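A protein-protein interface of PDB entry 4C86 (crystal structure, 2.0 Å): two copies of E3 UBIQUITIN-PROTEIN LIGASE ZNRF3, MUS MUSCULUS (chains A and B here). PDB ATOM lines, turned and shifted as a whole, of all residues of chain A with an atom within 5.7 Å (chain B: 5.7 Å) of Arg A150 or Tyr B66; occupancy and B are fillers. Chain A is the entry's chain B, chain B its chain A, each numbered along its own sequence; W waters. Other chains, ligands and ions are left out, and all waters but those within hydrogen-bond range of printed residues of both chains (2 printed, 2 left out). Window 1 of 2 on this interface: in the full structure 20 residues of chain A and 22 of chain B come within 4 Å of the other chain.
The guanidinium group (NH2) of Arg A152 lies within hydrogen-bond range of the side-chain hydroxyl (OH) of Tyr B66 (2.6 Å). The guanidinium group (NE) of Arg A152 sits close to the guanidinium group (NH1) of Arg B126, at 3.5 Å. OE1 of Glu A43 is in salt-bridge range of NH2 of Arg B126 (3.8 Å). The guanidinium group (NH2) of Arg B150 sits close to the guanidinium group (NH2) of Arg A150, 3.4 Å away. NH2 of Arg A150 lies within hydrogen-bond range of O of Glu B43 (3.1 Å). The side-chain carboxylate of Glu A43 is in hydrogen-bond range of the backbone NH of Glu B43, 3.0 Å away. The backbone carbonyl oxygen of Gly B67 sits at hydrogen-bond distance from the guanidinium group of Arg A150 (3.2 Å). The backbone NH (N) of Tyr B66 sits at hydrogen-bond distance from the side-chain hydroxyl (OH) of Tyr A22, at 2.8 Å. O of Tyr B64 sits at hydrogen-bond distance from OH of Tyr A22, 2.8 Å away. The side-chain hydroxyl of Thr B100 lies within hydrogen-bond range of the side-chain carboxylate of Glu A43 (2.7 Å). The backbone carbonyl oxygen (O) of Glu A43 is in hydrogen-bond range of the guanidinium group (NH2) of Arg B150, at 3.0 Å.
The backbone carbonyl oxygen (O) of Trp B68 lies within hydrogen-bond range of the backbone NH (N) of Thr B100, at 2.7 Å. N of Val A12 lies within hydrogen-bond range of O of Arg A150 (2.8 Å). The side-chain carboxylate of Glu A43 is in salt-bridge range of the guanidinium group of Arg A150, 2.9 Å away. The backbone NH (N) of Gly B67 is in hydrogen-bond range of the backbone carbonyl oxygen (O) of Gly B98 (2.7 Å). The backbone carbonyl oxygen (O) of Thr B100 lies within hydrogen-bond range of the guanidinium group (NE) of Arg B126. The indole nitrogen of Trp B68 sits close to the backbone carbonyl oxygen of Gly B98 (3.4 Å).
Tyr B66 touches Val A12 (CE2 to CG1, 3.8 Å). Phe A14 touches Tyr B66. Glu B65 touches Tyr A22 (C to OH, 3.4 Å). Tyr A22 touches Gly B98. Arg B150 touches Gly A44. CA of Gly B44 touches NH2 of Arg A150, at 3.5 Å. Arg A150 touches Tyr B66 (NH1 to O, 3.6 Å).
Arg A150 touches just these residues of chain B: Glu B43 (3.1 Å), Gly B44 (3.5 Å), Tyr B66 (3.6 Å), Gly B67 (3.2 Å) and Arg B150 (3.4 Å). Tyr B66 touches five residues of chain A. Of the printed residues of chain A, Arg B126 touches Glu A43 and Arg A152. Of the printed residues of chain A, Gly B67 touches Arg A150. The nearest residue of chain B that does not touch Arg A150 is Glu B45 (4.8 Å). The nearest residue of chain A that does not touch Tyr B66 is Thr A24 (4.1 Å).
Hydrophobic or aromatic side chains of chain A that line the printed part of chain B: Val A12, Phe A14 and Tyr A22. Among the printed residues, 18 pairs touch across the chains.
Glu B43 touches its own counterpart, Glu A43. Glu A43 touches Arg B150, and with the chains exchanged Arg A150 touches Glu B43. Gly A44 touches Arg B150, and with the chains exchanged Arg A150 touches Gly B44. Arg B150 touches its own counterpart, Arg A150. 4 positions are printed for both chains. Of the 18 pairs that touch across the chains among the printed residues, 6 have their exchanged pair printed and touching as well.
Water W2 lies within hydrogen-bond range of the guanidinium group of Arg B126 and the guanidinium group of Arg A152. Water W1 lies within hydrogen-bond range of the guanidinium group (NH1) of Arg A150 (2.9 Å) and the backbone carbonyl oxygen (O) of Tyr B66 (3.0 Å).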
ATOM      1  N   GLU A  10      12.174  15.559  -6.501  1.00  0.00           N
ATOM      2  CA  GLU A  10      12.997  16.061  -7.608  1.00  0.00           C
ATOM      3  C   GLU A  10      13.660  17.392  -7.230  1.00  0.00           C
ATOM      4  O   GLU A  10      13.015  18.286  -6.689  1.00  0.00           O
ATOM      5  CB  GLU A  10      12.145  16.288  -8.824  1.00  0.00           C
ATOM      6  CG  GLU A  10      11.698  15.033  -9.540  1.00  0.00           C
ATOM      7  CD  GLU A  10      10.792  15.319 -10.726  1.00  0.00           C
ATOM      8  OE1 GLU A  10      10.205  16.426 -10.794  1.00  0.00           O
ATOM      9  OE2 GLU A  10      10.674  14.433 -11.613  1.00  0.00           O
ATOM     10  N   VAL A  11      14.949  17.505  -7.505  1.00  0.00           N
ATOM     11  CA  VAL A  11      15.685  18.729  -7.246  1.00  0.00           C
ATOM     12  C   VAL A  11      16.035  19.215  -8.642  1.00  0.00           C
ATOM     13  O   VAL A  11      16.667  18.510  -9.462  1.00  0.00           O
ATOM     14  CB  VAL A  11      16.936  18.492  -6.359  1.00  0.00           C
ATOM     15  CG1 VAL A  11      17.820  19.714  -6.288  1.00  0.00           C
ATOM     16  CG2 VAL A  11      16.545  18.088  -4.966  1.00  0.00           C
ATOM     17  N   VAL A  12      15.503  20.363  -8.976  1.00  0.00           N
ATOM     18  CA  VAL A  12      15.725  20.959 -10.288  1.00  0.00           C
ATOM     19  C   VAL A  12      16.653  22.153 -10.123  1.00  0.00           C
ATOM     20  O   VAL A  12      16.292  23.084  -9.438  1.00  0.00           O
ATOM     21  CB  VAL A  12      14.409  21.456 -10.878  1.00  0.00           C
ATOM     22  CG1 VAL A  12      14.587  21.994 -12.289  1.00  0.00           C
ATOM     23  CG2 VAL A  12      13.355  20.359 -10.823  1.00  0.00           C
ATOM     24  N   LEU A  13      17.844  22.105 -10.728  1.00  0.00           N
ATOM     25  CA  LEU A  13      18.676  23.298 -10.931  1.00  0.00           C
ATOM     26  C   LEU A  13      18.264  23.988 -12.200  1.00  0.00           C
ATOM     27  O   LEU A  13      18.020  23.319 -13.215  1.00  0.00           O
ATOM     28  CB  LEU A  13      20.154  22.927 -11.076  1.00  0.00           C
ATOM     29  CG  LEU A  13      20.764  22.278  -9.842  1.00  0.00           C
ATOM     30  CD1 LEU A  13      22.069  21.597 -10.198  1.00  0.00           C
ATOM     31  CD2 LEU A  13      20.943  23.245  -8.703  1.00  0.00           C
ATOM     32  N   PHE A  14      18.237  25.321 -12.180  1.00  0.00           N
ATOM     33  CA  PHE A  14      17.816  26.084 -13.351  1.00  0.00           C
ATOM     34  C   PHE A  14      18.652  27.332 -13.633  1.00  0.00           C
ATOM     35  O   PHE A  14      19.242  27.931 -12.737  1.00  0.00           O
ATOM     36  CB  PHE A  14      16.344  26.506 -13.216  1.00  0.00           C
ATOM     37  CG  PHE A  14      16.053  27.320 -11.995  1.00  0.00           C
ATOM     38  CD1 PHE A  14      15.700  26.700 -10.807  1.00  0.00           C
ATOM     39  CD2 PHE A  14      16.116  28.719 -12.034  1.00  0.00           C
ATOM     40  CE1 PHE A  14      15.442  27.451  -9.678  1.00  0.00           C
ATOM     41  CE2 PHE A  14      15.833  29.481 -10.914  1.00  0.00           C
ATOM     42  CZ  PHE A  14      15.509  28.848  -9.730  1.00  0.00           C
ATOM     43  N   TYR A  22      15.104  28.283 -20.708  1.00  0.00           N
ATOM     44  CA  TYR A  22      15.564  27.736 -19.415  1.00  0.00           C
ATOM     45  C   TYR A  22      16.383  26.463 -19.681  1.00  0.00           C
ATOM     46  O   TYR A  22      15.977  25.589 -20.477  1.00  0.00           O
ATOM     47  CB  TYR A  22      14.405  27.435 -18.449  1.00  0.00           C
ATOM     48  CG  TYR A  22      14.165  28.452 -17.334  1.00  0.00           C
ATOM     49  CD1 TYR A  22      15.145  28.739 -16.390  1.00  0.00           C
ATOM     50  CD2 TYR A  22      12.944  29.076 -17.191  1.00  0.00           C
ATOM     51  CE1 TYR A  22      14.916  29.664 -15.385  1.00  0.00           C
ATOM     52  CE2 TYR A  22      12.706  29.985 -16.175  1.00  0.00           C
ATOM     53  CZ  TYR A  22      13.694  30.272 -15.275  1.00  0.00           C
ATOM     54  OH  TYR A  22      13.471  31.185 -14.257  1.00  0.00           O
ATOM     55  N   THR A  24      17.699  23.289 -17.578  1.00  0.00           N
ATOM     56  CA  THR A  24      17.406  22.619 -16.321  1.00  0.00           C
ATOM     57  C   THR A  24      18.256  21.364 -16.137  1.00  0.00           C
ATOM     58  O   THR A  24      18.828  20.847 -17.095  1.00  0.00           O
ATOM     59  CB  THR A  24      15.919  22.239 -16.220  1.00  0.00           C
ATOM     60  OG1 THR A  24      15.514  21.535 -17.390  1.00  0.00           O
ATOM     61  CG2 THR A  24      15.061  23.420 -16.027  1.00  0.00           C
ATOM     62  N   GLU A  43       6.097  22.038  -3.112  1.00  0.00           N
ATOM     63  CA  GLU A  43       7.112  22.482  -4.052  1.00  0.00           C
ATOM     64  C   GLU A  43       7.538  23.903  -3.651  1.00  0.00           C
ATOM     65  O   GLU A  43       6.709  24.686  -3.210  1.00  0.00           O
ATOM     66  CB  GLU A  43       6.545  22.473  -5.471  1.00  0.00           C
ATOM     67  CG  GLU A  43       7.536  22.890  -6.555  1.00  0.00           C
ATOM     68  CD  GLU A  43       6.915  22.995  -7.954  1.00  0.00           C
ATOM     69  OE1 GLU A  43       5.743  22.553  -8.151  1.00  0.00           O
ATOM     70  OE2 GLU A  43       7.607  23.492  -8.884  1.00  0.00           O
ATOM     71  N   GLY A  44       8.824  24.199  -3.752  1.00  0.00           N
ATOM     72  CA  GLY A  44       9.305  25.572  -3.544  1.00  0.00           C
ATOM     73  C   GLY A  44      10.805  25.655  -3.643  1.00  0.00           C
ATOM     74  O   GLY A  44      11.502  24.655  -3.752  1.00  0.00           O
ATOM     75  N   GLU A  45      11.302  26.874  -3.586  1.00  0.00           N
ATOM     76  CA  GLU A  45      12.736  27.124  -3.653  1.00  0.00           C
ATOM     77  C   GLU A  45      13.381  26.526  -2.456  1.00  0.00           C
ATOM     78  O   GLU A  45      12.873  26.622  -1.345  1.00  0.00           O
ATOM     79  CB  GLU A  45      13.046  28.623  -3.712  1.00  0.00           C
ATOM     80  CG  GLU A  45      14.446  28.924  -4.250  1.00  0.00           C
ATOM     81  CD  GLU A  45      14.858  30.393  -4.081  1.00  0.00           C
ATOM     82  OE1 GLU A  45      13.994  31.228  -3.730  1.00  0.00           O
ATOM     83  OE2 GLU A  45      16.052  30.720  -4.299  1.00  0.00           O
ATOM     84  N   ILE A  46      14.514  25.881  -2.672  1.00  0.00           N
ATOM     85  CA  ILE A  46      15.268  25.294  -1.586  1.00  0.00           C
ATOM     86  C   ILE A  46      16.073  26.324  -0.835  1.00  0.00           C
ATOM     87  O   ILE A  46      16.741  27.181  -1.426  1.00  0.00           O
ATOM     88  CB  ILE A  46      16.249  24.227  -2.070  1.00  0.00           C
ATOM     89  CG1 ILE A  46      15.491  23.013  -2.580  1.00  0.00           C
ATOM     90  CG2 ILE A  46      17.165  23.817  -0.935  1.00  0.00           C
ATOM     91  CD1 ILE A  46      16.321  22.048  -3.362  1.00  0.00           C
ATOM     92  N   VAL A 148      20.753  28.253  -7.076  1.00  0.00           N
ATOM     93  CA  VAL A 148      19.341  28.258  -6.781  1.00  0.00           C
ATOM     94  C   VAL A 148      18.791  26.910  -7.322  1.00  0.00           C
ATOM     95  O   VAL A 148      19.196  26.430  -8.378  1.00  0.00           O
ATOM     96  CB  VAL A 148      18.635  29.474  -7.424  1.00  0.00           C
ATOM     97  CG1 VAL A 148      19.290  30.776  -6.973  1.00  0.00           C
ATOM     98  CG2 VAL A 148      18.677  29.432  -8.954  1.00  0.00           C
ATOM     99  N   ALA A 149      17.894  26.309  -6.566  1.00  0.00           N
ATOM    100  CA  ALA A 149      17.361  24.959  -6.864  1.00  0.00           C
ATOM    101  C   ALA A 149      15.927  24.977  -6.343  1.00  0.00           C
ATOM    102  O   ALA A 149      15.606  25.653  -5.329  1.00  0.00           O
ATOM    103  CB  ALA A 149      18.197  23.869  -6.179  1.00  0.00           C
ATOM    104  N   ARG A 150      15.043  24.346  -7.088  1.00  0.00           N
ATOM    105  CA  ARG A 150      13.704  24.073  -6.618  1.00  0.00           C
ATOM    106  C   ARG A 150      13.584  22.587  -6.262  1.00  0.00           C
ATOM    107  O   ARG A 150      14.191  21.708  -6.916  1.00  0.00           O
ATOM    108  CB  ARG A 150      12.702  24.436  -7.704  1.00  0.00           C
ATOM    109  CG  ARG A 150      11.331  24.731  -7.174  1.00  0.00           C
ATOM    110  CD  ARG A 150      10.424  25.234  -8.258  1.00  0.00           C
ATOM    111  NE  ARG A 150       9.127  25.626  -7.734  1.00  0.00           N
ATOM    112  CZ  ARG A 150       8.875  26.737  -7.053  1.00  0.00           C
ATOM    113  NH1 ARG A 150       9.842  27.611  -6.787  1.00  0.00           N
ATOM    114  NH2 ARG A 150       7.639  26.969  -6.639  1.00  0.00           N
ATOM    115  N   ALA A 151      12.833  22.307  -5.205  1.00  0.00           N
ATOM    116  CA  ALA A 151      12.498  20.943  -4.828  1.00  0.00           C
ATOM    117  C   ALA A 151      11.006  20.684  -5.076  1.00  0.00           C
ATOM    118  O   ALA A 151      10.168  21.507  -4.792  1.00  0.00           O
ATOM    119  CB  ALA A 151      12.823  20.710  -3.377  1.00  0.00           C
ATOM    120  N   ARG A 152      10.716  19.560  -5.687  1.00  0.00           N
ATOM    121  CA  ARG A 152       9.343  19.158  -5.913  1.00  0.00           C
ATOM    122  C   ARG A 152       9.128  17.919  -5.067  1.00  0.00           C
ATOM    123  O   ARG A 152       9.854  16.949  -5.194  1.00  0.00           O
ATOM    124  CB  ARG A 152       9.111  18.818  -7.402  1.00  0.00           C
ATOM    125  CG  ARG A 152       9.451  19.937  -8.387  1.00  0.00           C
ATOM    126  CD  ARG A 152       8.656  19.733  -9.656  1.00  0.00           C
ATOM    127  NE  ARG A 152       9.141  20.463 -10.818  1.00  0.00           N
ATOM    128  CZ  ARG A 152       9.859  19.939 -11.807  1.00  0.00           C
ATOM    129  NH1 ARG A 152      10.281  18.665 -11.792  1.00  0.00           N
ATOM    130  NH2 ARG A 152      10.187  20.717 -12.825  1.00  0.00           N
ATOM    131  N   GLU B  43       3.062  23.459  -7.057  1.00  0.00           N
ATOM    132  CA  GLU B  43       2.883  24.598  -6.191  1.00  0.00           C
ATOM    133  C   GLU B  43       3.873  25.685  -6.624  1.00  0.00           C
ATOM    134  O   GLU B  43       5.013  25.407  -6.992  1.00  0.00           O
ATOM    135  CB  GLU B  43       3.153  24.182  -4.747  1.00  0.00           C
ATOM    136  CG  GLU B  43       3.501  25.325  -3.824  1.00  0.00           C
ATOM    137  CD  GLU B  43       3.689  24.926  -2.368  1.00  0.00           C
ATOM    138  OE1 GLU B  43       3.767  23.694  -2.054  1.00  0.00           O
ATOM    139  OE2 GLU B  43       3.786  25.874  -1.544  1.00  0.00           O
ATOM    140  N   GLY B  44       3.431  26.932  -6.549  1.00  0.00           N
ATOM    141  CA  GLY B  44       4.335  28.052  -6.791  1.00  0.00           C
ATOM    142  C   GLY B  44       3.569  29.337  -6.767  1.00  0.00           C
ATOM    143  O   GLY B  44       2.355  29.363  -6.648  1.00  0.00           O
ATOM    144  N   GLU B  45       4.277  30.416  -6.957  1.00  0.00           N
ATOM    145  CA  GLU B  45       3.661  31.718  -6.866  1.00  0.00           C
ATOM    146  C   GLU B  45       2.902  31.972  -8.118  1.00  0.00           C
ATOM    147  O   GLU B  45       3.366  31.655  -9.194  1.00  0.00           O
ATOM    148  CB  GLU B  45       4.747  32.743  -6.670  1.00  0.00           C
ATOM    149  CG  GLU B  45       4.288  34.172  -6.532  1.00  0.00           C
ATOM    150  CD  GLU B  45       5.493  35.062  -6.477  1.00  0.00           C
ATOM    151  OE1 GLU B  45       6.478  34.616  -5.858  1.00  0.00           O
ATOM    152  OE2 GLU B  45       5.474  36.170  -7.069  1.00  0.00           O
ATOM    153  N   TYR B  64      10.235  33.690 -16.314  1.00  0.00           N
ATOM    154  CA  TYR B  64       9.967  34.044 -14.899  1.00  0.00           C
ATOM    155  C   TYR B  64      10.631  33.085 -13.948  1.00  0.00           C
ATOM    156  O   TYR B  64      10.757  31.909 -14.279  1.00  0.00           O
ATOM    157  CB  TYR B  64       8.465  34.091 -14.619  1.00  0.00           C
ATOM    158  CG  TYR B  64       7.764  35.068 -15.518  1.00  0.00           C
ATOM    159  CD1 TYR B  64       8.414  36.250 -15.941  1.00  0.00           C
ATOM    160  CD2 TYR B  64       6.480  34.823 -15.976  1.00  0.00           C
ATOM    161  CE1 TYR B  64       7.787  37.149 -16.778  1.00  0.00           C
ATOM    162  CE2 TYR B  64       5.848  35.726 -16.811  1.00  0.00           C
ATOM    163  CZ  TYR B  64       6.499  36.887 -17.201  1.00  0.00           C
ATOM    164  OH  TYR B  64       5.875  37.785 -18.037  1.00  0.00           O
ATOM    165  N   GLU B  65      11.063  33.602 -12.790  1.00  0.00           N
ATOM    166  CA  GLU B  65      11.725  32.812 -11.742  1.00  0.00           C
ATOM    167  C   GLU B  65      11.157  31.380 -11.715  1.00  0.00           C
ATOM    168  O   GLU B  65       9.993  31.197 -11.472  1.00  0.00           O
ATOM    169  CB  GLU B  65      11.559  33.481 -10.353  1.00  0.00           C
ATOM    170  CG  GLU B  65      12.086  32.644  -9.175  1.00  0.00           C
ATOM    171  CD  GLU B  65      11.766  33.224  -7.794  1.00  0.00           C
ATOM    172  OE1 GLU B  65      12.512  34.113  -7.323  1.00  0.00           O
ATOM    173  OE2 GLU B  65      10.779  32.780  -7.153  1.00  0.00           O
ATOM    174  N   TYR B  66      11.989  30.393 -11.981  1.00  0.00           N
ATOM    175  CA  TYR B  66      11.539  29.015 -12.210  1.00  0.00           C
ATOM    176  C   TYR B  66      10.514  28.614 -11.182  1.00  0.00           C
ATOM    177  O   TYR B  66      10.667  28.916  -9.985  1.00  0.00           O
ATOM    178  CB  TYR B  66      12.715  28.049 -12.148  1.00  0.00           C
ATOM    179  CG  TYR B  66      12.316  26.666 -12.582  1.00  0.00           C
ATOM    180  CD1 TYR B  66      12.159  26.378 -13.934  1.00  0.00           C
ATOM    181  CD2 TYR B  66      12.044  25.649 -11.644  1.00  0.00           C
ATOM    182  CE1 TYR B  66      11.773  25.120 -14.361  1.00  0.00           C
ATOM    183  CE2 TYR B  66      11.661  24.381 -12.067  1.00  0.00           C
ATOM    184  CZ  TYR B  66      11.523  24.129 -13.421  1.00  0.00           C
ATOM    185  OH  TYR B  66      11.154  22.885 -13.880  1.00  0.00           O
ATOM    186  N   GLY B  67       9.434  27.981 -11.633  1.00  0.00           N
ATOM    187  CA  GLY B  67       8.493  27.349 -10.689  1.00  0.00           C
ATOM    188  C   GLY B  67       7.218  28.069 -10.394  1.00  0.00           C
ATOM    189  O   GLY B  67       6.496  27.717  -9.480  1.00  0.00           O
ATOM    190  N   TRP B  68       6.931  29.121 -11.153  1.00  0.00           N
ATOM    191  CA  TRP B  68       5.689  29.825 -10.997  1.00  0.00           C
ATOM    192  C   TRP B  68       4.492  29.031 -11.561  1.00  0.00           C
ATOM    193  O   TRP B  68       4.638  28.128 -12.402  1.00  0.00           O
ATOM    194  CB  TRP B  68       5.757  31.180 -11.723  1.00  0.00           C
ATOM    195  CG  TRP B  68       6.244  31.104 -13.100  1.00  0.00           C
ATOM    196  CD1 TRP B  68       7.559  30.953 -13.522  1.00  0.00           C
ATOM    197  CD2 TRP B  68       5.471  31.247 -14.279  1.00  0.00           C
ATOM    198  NE1 TRP B  68       7.608  30.929 -14.871  1.00  0.00           N
ATOM    199  CE2 TRP B  68       6.350  31.153 -15.364  1.00  0.00           C
ATOM    200  CE3 TRP B  68       4.104  31.452 -14.529  1.00  0.00           C
ATOM    201  CZ2 TRP B  68       5.912  31.245 -16.697  1.00  0.00           C
ATOM    202  CZ3 TRP B  68       3.686  31.558 -15.817  1.00  0.00           C
ATOM    203  CH2 TRP B  68       4.591  31.465 -16.898  1.00  0.00           C
ATOM    204  N   VAL B  95       5.277  26.429 -19.727  1.00  0.00           N
ATOM    205  CA  VAL B  95       6.220  25.547 -19.095  1.00  0.00           C
ATOM    206  C   VAL B  95       7.660  25.848 -19.558  1.00  0.00           C
ATOM    207  O   VAL B  95       8.567  25.787 -18.776  1.00  0.00           O
ATOM    208  CB  VAL B  95       5.915  24.054 -19.354  1.00  0.00           C
ATOM    209  CG1 VAL B  95       7.060  23.198 -18.888  1.00  0.00           C
ATOM    210  CG2 VAL B  95       4.598  23.623 -18.674  1.00  0.00           C
ATOM    211  N   GLY B  98       9.271  28.488 -17.603  1.00  0.00           N
ATOM    212  CA  GLY B  98       9.460  28.158 -16.211  1.00  0.00           C
ATOM    213  C   GLY B  98       8.239  27.813 -15.343  1.00  0.00           C
ATOM    214  O   GLY B  98       8.398  27.657 -14.124  1.00  0.00           O
ATOM    215  N   ALA B  99       7.042  27.723 -15.941  1.00  0.00           N
ATOM    216  CA  ALA B  99       5.833  27.446 -15.187  1.00  0.00           C
ATOM    217  C   ALA B  99       5.876  25.977 -14.679  1.00  0.00           C
ATOM    218  O   ALA B  99       6.132  25.062 -15.443  1.00  0.00           O
ATOM    219  CB  ALA B  99       4.599  27.664 -16.030  1.00  0.00           C
ATOM    220  N   THR B 100       5.633  25.791 -13.405  1.00  0.00           N
ATOM    221  CA  THR B 100       5.534  24.443 -12.834  1.00  0.00           C
ATOM    222  C   THR B 100       4.111  23.880 -13.168  1.00  0.00           C
ATOM    223  O   THR B 100       3.891  22.688 -13.165  1.00  0.00           O
ATOM    224  CB  THR B 100       5.828  24.414 -11.303  1.00  0.00           C
ATOM    225  OG1 THR B 100       5.815  23.052 -10.846  1.00  0.00           O
ATOM    226  CG2 THR B 100       4.771  25.201 -10.451  1.00  0.00           C
ATOM    227  N   ARG B 126       4.367  18.574 -16.958  1.00  0.00           N
ATOM    228  CA  ARG B 126       3.758  19.385 -15.887  1.00  0.00           C
ATOM    229  C   ARG B 126       2.219  19.396 -15.978  1.00  0.00           C
ATOM    230  O   ARG B 126       1.661  19.151 -17.064  1.00  0.00           O
ATOM    231  CB  ARG B 126       4.284  20.831 -15.975  1.00  0.00           C
ATOM    232  CG  ARG B 126       5.796  21.032 -15.855  1.00  0.00           C
ATOM    233  CD  ARG B 126       6.407  20.355 -14.652  1.00  0.00           C
ATOM    234  NE  ARG B 126       5.779  20.712 -13.382  1.00  0.00           N
ATOM    235  CZ  ARG B 126       5.792  19.966 -12.269  1.00  0.00           C
ATOM    236  NH1 ARG B 126       6.436  18.809 -12.204  1.00  0.00           N
ATOM    237  NH2 ARG B 126       5.183  20.398 -11.185  1.00  0.00           N
ATOM    238  N   ARG B 150       0.068  32.474  -3.755  1.00  0.00           N
ATOM    239  CA  ARG B 150       0.718  31.201  -4.010  1.00  0.00           C
ATOM    240  C   ARG B 150      -0.361  30.127  -4.193  1.00  0.00           C
ATOM    241  O   ARG B 150      -1.326  30.048  -3.401  1.00  0.00           O
ATOM    242  CB  ARG B 150       1.674  30.840  -2.876  1.00  0.00           C
ATOM    243  CG  ARG B 150       2.537  29.610  -3.138  1.00  0.00           C
ATOM    244  CD  ARG B 150       3.581  29.393  -2.046  1.00  0.00           C
ATOM    245  NE  ARG B 150       4.584  28.408  -2.442  1.00  0.00           N
ATOM    246  CZ  ARG B 150       5.665  28.653  -3.157  1.00  0.00           C
ATOM    247  NH1 ARG B 150       5.961  29.883  -3.536  1.00  0.00           N
ATOM    248  NH2 ARG B 150       6.471  27.652  -3.519  1.00  0.00           N
HETATM  249  O   HOH W   1      12.523  28.278  -7.756  1.00  0.00           O
HETATM  250  O   HOH W   2       8.201  17.438 -14.006  1.00  0.00           O
